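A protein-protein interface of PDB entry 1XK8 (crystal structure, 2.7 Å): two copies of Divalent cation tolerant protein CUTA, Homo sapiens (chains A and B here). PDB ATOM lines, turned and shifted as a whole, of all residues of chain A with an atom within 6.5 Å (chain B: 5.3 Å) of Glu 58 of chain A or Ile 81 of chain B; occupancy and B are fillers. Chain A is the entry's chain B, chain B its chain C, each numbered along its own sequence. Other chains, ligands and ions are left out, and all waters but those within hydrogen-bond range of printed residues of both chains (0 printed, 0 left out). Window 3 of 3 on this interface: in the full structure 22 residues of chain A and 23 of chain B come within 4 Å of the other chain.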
ATOM      1  N   ALA A  53      16.130  11.829  -7.471  1.00  0.00           N
ATOM      2  CA  ALA A  53      16.269  10.477  -8.001  1.00  0.00           C
ATOM      3  C   ALA A  53      14.929   9.777  -8.120  1.00  0.00           C
ATOM      4  O   ALA A  53      14.589   9.241  -9.180  1.00  0.00           O
ATOM      5  CB  ALA A  53      17.182   9.661  -7.111  1.00  0.00           C
ATOM      6  N   ARG A  54      14.174   9.767  -7.022  1.00  0.00           N
ATOM      7  CA  ARG A  54      12.855   9.136  -7.015  1.00  0.00           C
ATOM      8  C   ARG A  54      11.931   9.789  -8.060  1.00  0.00           C
ATOM      9  O   ARG A  54      11.232   9.097  -8.789  1.00  0.00           O
ATOM     10  CB  ARG A  54      12.255   9.163  -5.608  1.00  0.00           C
ATOM     11  CG  ARG A  54      13.014   8.241  -4.610  1.00  0.00           C
ATOM     12  CD  ARG A  54      12.237   8.021  -3.302  1.00  0.00           C
ATOM     13  NE  ARG A  54      11.066   7.132  -3.487  1.00  0.00           N
ATOM     14  CZ  ARG A  54      10.936   5.886  -2.996  1.00  0.00           C
ATOM     15  NH1 ARG A  54      11.893   5.325  -2.249  1.00  0.00           N
ATOM     16  NH2 ARG A  54       9.822   5.194  -3.237  1.00  0.00           N
ATOM     17  N   ALA A  55      11.975  11.113  -8.158  1.00  0.00           N
ATOM     18  CA  ALA A  55      11.126  11.842  -9.109  1.00  0.00           C
ATOM     19  C   ALA A  55      11.409  11.453 -10.567  1.00  0.00           C
ATOM     20  O   ALA A  55      10.488  11.093 -11.296  1.00  0.00           O
ATOM     21  CB  ALA A  55      11.282  13.336  -8.923  1.00  0.00           C
ATOM     22  N   VAL A  56      12.677  11.514 -10.986  1.00  0.00           N
ATOM     23  CA  VAL A  56      13.023  11.226 -12.399  1.00  0.00           C
ATOM     24  C   VAL A  56      12.642   9.812 -12.821  1.00  0.00           C
ATOM     25  O   VAL A  56      12.261   9.592 -13.968  1.00  0.00           O
ATOM     26  CB  VAL A  56      14.538  11.454 -12.749  1.00  0.00           C
ATOM     27  CG1 VAL A  56      14.886  12.940 -12.684  1.00  0.00           C
ATOM     28  CG2 VAL A  56      15.470  10.618 -11.863  1.00  0.00           C
ATOM     29  N   VAL A  57      12.754   8.859 -11.896  1.00  0.00           N
ATOM     30  CA  VAL A  57      12.362   7.470 -12.162  1.00  0.00           C
ATOM     31  C   VAL A  57      10.843   7.363 -12.247  1.00  0.00           C
ATOM     32  O   VAL A  57      10.314   6.761 -13.173  1.00  0.00           O
ATOM     33  CB  VAL A  57      12.886   6.505 -11.079  1.00  0.00           C
ATOM     34  CG1 VAL A  57      12.432   5.089 -11.365  1.00  0.00           C
ATOM     35  CG2 VAL A  57      14.387   6.556 -11.021  1.00  0.00           C
ATOM     36  N   GLU A  58      10.158   7.966 -11.281  1.00  0.00           N
ATOM     37  CA  GLU A  58       8.694   7.988 -11.235  1.00  0.00           C
ATOM     38  C   GLU A  58       8.090   8.664 -12.463  1.00  0.00           C
ATOM     39  O   GLU A  58       7.071   8.222 -12.984  1.00  0.00           O
ATOM     40  CB  GLU A  58       8.276   8.740  -9.990  1.00  0.00           C
ATOM     41  CG  GLU A  58       6.941   8.402  -9.444  1.00  0.00           C
ATOM     42  CD  GLU A  58       6.738   9.068  -8.100  1.00  0.00           C
ATOM     43  OE1 GLU A  58       5.565   9.363  -7.757  1.00  0.00           O
ATOM     44  OE2 GLU A  58       7.766   9.313  -7.397  1.00  0.00           O
ATOM     45  N   LYS A  59       8.736   9.730 -12.923  1.00  0.00           N
ATOM     46  CA  LYS A  59       8.314  10.450 -14.135  1.00  0.00           C
ATOM     47  C   LYS A  59       8.813   9.774 -15.446  1.00  0.00           C
ATOM     48  O   LYS A  59       8.593  10.303 -16.538  1.00  0.00           O
ATOM     49  CB  LYS A  59       8.806  11.912 -14.075  1.00  0.00           C
ATOM     50  CG  LYS A  59       8.518  12.657 -12.738  1.00  0.00           C
ATOM     51  CD  LYS A  59       7.639  13.913 -12.877  1.00  0.00           C
ATOM     52  CE  LYS A  59       7.094  14.344 -11.482  1.00  0.00           C
ATOM     53  NZ  LYS A  59       7.173  15.819 -11.239  1.00  0.00           N
ATOM     54  N   ARG A  60       9.483   8.619 -15.328  1.00  0.00           N
ATOM     55  CA  ARG A  60       9.983   7.867 -16.494  1.00  0.00           C
ATOM     56  C   ARG A  60      11.095   8.584 -17.285  1.00  0.00           C
ATOM     57  O   ARG A  60      11.368   8.233 -18.437  1.00  0.00           O
ATOM     58  N   LEU A  61      11.743   9.568 -16.658  1.00  0.00           N
ATOM     59  CA  LEU A  61      12.857  10.316 -17.281  1.00  0.00           C
ATOM     60  C   LEU A  61      14.197   9.569 -17.180  1.00  0.00           C
ATOM     61  O   LEU A  61      15.164   9.919 -17.866  1.00  0.00           O
ATOM     62  CB  LEU A  61      12.997  11.701 -16.637  1.00  0.00           C
ATOM     63  CG  LEU A  61      12.082  12.778 -17.232  1.00  0.00           C
ATOM     64  CD1 LEU A  61      10.695  12.629 -16.738  1.00  0.00           C
ATOM     65  CD2 LEU A  61      12.586  14.174 -16.911  1.00  0.00           C
ATOM     66  N   ALA A  62      14.237   8.548 -16.322  1.00  0.00           N
ATOM     67  CA  ALA A  62      15.419   7.729 -16.152  1.00  0.00           C
ATOM     68  C   ALA A  62      15.029   6.296 -15.808  1.00  0.00           C
ATOM     69  O   ALA A  62      13.987   6.059 -15.186  1.00  0.00           O
ATOM     70  CB  ALA A  62      16.287   8.304 -15.062  1.00  0.00           C
ATOM     71  N   ILE B  74      18.447   3.442  -7.231  1.00  0.00           N
ATOM     72  CA  ILE B  74      17.020   3.771  -7.227  1.00  0.00           C
ATOM     73  C   ILE B  74      16.407   3.444  -8.583  1.00  0.00           C
ATOM     74  O   ILE B  74      16.733   4.055  -9.582  1.00  0.00           O
ATOM     75  CB  ILE B  74      16.773   5.243  -6.841  1.00  0.00           C
ATOM     76  CG1 ILE B  74      17.154   5.461  -5.371  1.00  0.00           C
ATOM     77  CG2 ILE B  74      15.295   5.622  -7.033  1.00  0.00           C
ATOM     78  CD1 ILE B  74      17.462   6.919  -5.000  1.00  0.00           C
ATOM     79  N   TYR B  75      15.499   2.477  -8.585  1.00  0.00           N
ATOM     80  CA  TYR B  75      14.851   1.999  -9.804  1.00  0.00           C
ATOM     81  C   TYR B  75      13.434   1.530  -9.487  1.00  0.00           C
ATOM     82  O   TYR B  75      13.060   1.389  -8.300  1.00  0.00           O
ATOM     83  CB  TYR B  75      15.674   0.880 -10.450  1.00  0.00           C
ATOM     84  CG  TYR B  75      15.951  -0.290  -9.543  1.00  0.00           C
ATOM     85  CD1 TYR B  75      15.182  -1.458  -9.619  1.00  0.00           C
ATOM     86  CD2 TYR B  75      16.991  -0.243  -8.607  1.00  0.00           C
ATOM     87  CE1 TYR B  75      15.438  -2.548  -8.780  1.00  0.00           C
ATOM     88  CE2 TYR B  75      17.255  -1.326  -7.754  1.00  0.00           C
ATOM     89  CZ  TYR B  75      16.476  -2.474  -7.843  1.00  0.00           C
ATOM     90  OH  TYR B  75      16.739  -3.555  -7.007  1.00  0.00           O
ATOM     91  N   GLU B  76      12.638   1.345 -10.550  1.00  0.00           N
ATOM     92  CA  GLU B  76      11.275   0.789 -10.434  1.00  0.00           C
ATOM     93  C   GLU B  76      11.265  -0.677 -10.834  1.00  0.00           C
ATOM     94  O   GLU B  76      12.168  -1.174 -11.531  1.00  0.00           O
ATOM     95  CB  GLU B  76      10.234   1.569 -11.276  1.00  0.00           C
ATOM     96  CG  GLU B  76       9.343   2.548 -10.467  1.00  0.00           C
ATOM     97  CD  GLU B  76       8.163   3.134 -11.288  1.00  0.00           C
ATOM     98  OE1 GLU B  76       7.883   2.623 -12.401  1.00  0.00           O
ATOM     99  OE2 GLU B  76       7.516   4.108 -10.808  1.00  0.00           O
ATOM    100  N   GLY B  79       6.205  -1.083 -11.079  1.00  0.00           N
ATOM    101  CA  GLY B  79       5.636   0.247 -10.802  1.00  0.00           C
ATOM    102  C   GLY B  79       5.856   0.817  -9.403  1.00  0.00           C
ATOM    103  O   GLY B  79       5.241   1.840  -9.040  1.00  0.00           O
ATOM    104  N   LYS B  80       6.728   0.176  -8.616  1.00  0.00           N
ATOM    105  CA  LYS B  80       7.053   0.649  -7.261  1.00  0.00           C
ATOM    106  C   LYS B  80       8.548   0.940  -7.174  1.00  0.00           C
ATOM    107  O   LYS B  80       9.349   0.246  -7.802  1.00  0.00           O
ATOM    108  N   ILE B  81       8.931   1.952  -6.390  1.00  0.00           N
ATOM    109  CA  ILE B  81      10.310   2.419  -6.407  1.00  0.00           C
ATOM    110  C   ILE B  81      11.142   1.815  -5.284  1.00  0.00           C
ATOM    111  O   ILE B  81      10.843   2.018  -4.105  1.00  0.00           O
ATOM    112  CB  ILE B  81      10.373   3.966  -6.339  1.00  0.00           C
ATOM    113  CG1 ILE B  81       9.844   4.569  -7.642  1.00  0.00           C
ATOM    114  CG2 ILE B  81      11.816   4.457  -6.079  1.00  0.00           C
ATOM    115  CD1 ILE B  81       9.592   6.075  -7.572  1.00  0.00           C
ATOM    116  N   GLU B  82      12.213   1.110  -5.669  1.00  0.00           N
ATOM    117  CA  GLU B  82      13.123   0.415  -4.740  1.00  0.00           C
ATOM    118  C   GLU B  82      14.396   1.198  -4.459  1.00  0.00           C
ATOM    119  O   GLU B  82      14.876   1.920  -5.324  1.00  0.00           O
ATOM    120  CB  GLU B  82      13.636  -0.875  -5.398  1.00  0.00           C
ATOM    121  CG  GLU B  82      12.606  -1.895  -5.812  1.00  0.00           C
ATOM    122  CD  GLU B  82      12.784  -3.230  -5.083  1.00  0.00           C
ATOM    123  OE1 GLU B  82      11.748  -3.824  -4.683  1.00  0.00           O
ATOM    124  OE2 GLU B  82      13.962  -3.676  -4.906  1.00  0.00           O
ATOM    125  N   GLU B  83      14.968   0.995  -3.267  1.00  0.00           N
ATOM    126  CA  GLU B  83      16.306   1.497  -2.931  1.00  0.00           C
ATOM    127  C   GLU B  83      17.134   0.336  -2.398  1.00  0.00           C
ATOM    128  O   GLU B  83      16.716  -0.333  -1.441  1.00  0.00           O
ATOM    129  CB  GLU B  83      16.253   2.606  -1.874  1.00  0.00           C
ATOM    130  CG  GLU B  83      15.359   3.788  -2.231  1.00  0.00           C
ATOM    131  CD  GLU B  83      15.424   4.937  -1.201  1.00  0.00           C
ATOM    132  OE1 GLU B  83      14.635   5.895  -1.350  1.00  0.00           O
ATOM    133  OE2 GLU B  83      16.260   4.884  -0.255  1.00  0.00           O
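Of the printed residues of chain B, Val 57 of chain A touches Ile 74 (3.7 Å) and Glu 76 (3.8 Å). Glu 58 of chain A touches just one residue of chain B: Ile 81. Ala 62 of chain A touches none of the printed residues of chain B. Of the printed residues of chain A, Ile 74 of chain B touches Ala 53 and Val 57. Lys 80 of chain B touches none of the printed residues of chain A. Of the printed residues of chain A, Ile 81 of chain B touches Arg 54 and Glu 58.
No position is printed for both chains.
Printed residues of chain A that touch a printed residue of chain B: Ala 53, Arg 54, Val 57 and Glu 58. Hydrophobic or aromatic side chains of chain A within 4 Å of the printed part of chain B: Ala 53 and Val 57. Printed residues of chain B that touch a printed residue of chain A: Ile 74, Glu 76, Ile 81 and Glu 83. Hydrophobic or aromatic side chains of chain B within 4 Å of the printed part of chain A: Ile 74 and Ile 81. Along chain B the printed residues that touch a printed residue of chain A span positions 74 to 83. Among the printed residues, 6 pairs touch across the chains. Among the printed residues, Asp or Glu carboxylates within 4 Å of a Lys or Arg side-chain nitrogen of the other chain: Arg 54 of chain A with Glu 83 of chain B.
Among the printed residues, pairs that only touch across the chains: Ala 53 of chain A with Ile 74 of chain B (3.5 Å), Val 57 of chain A with Ile 74 of chain B (3.7 Å), Val 57 of chain A with Glu 76 of chain B (3.8 Å) and Glu 58 of chain A with Ile 81 of chain B (3.7 Å).
O of Ile 81 of chain B lies close to NH2 of Arg 54 of chain A, at 3.4 Å. OE1 of Glu 83 of chain B lies within salt-bridge range of NH1 of Arg 54 of chain A, at 2.9 Å.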
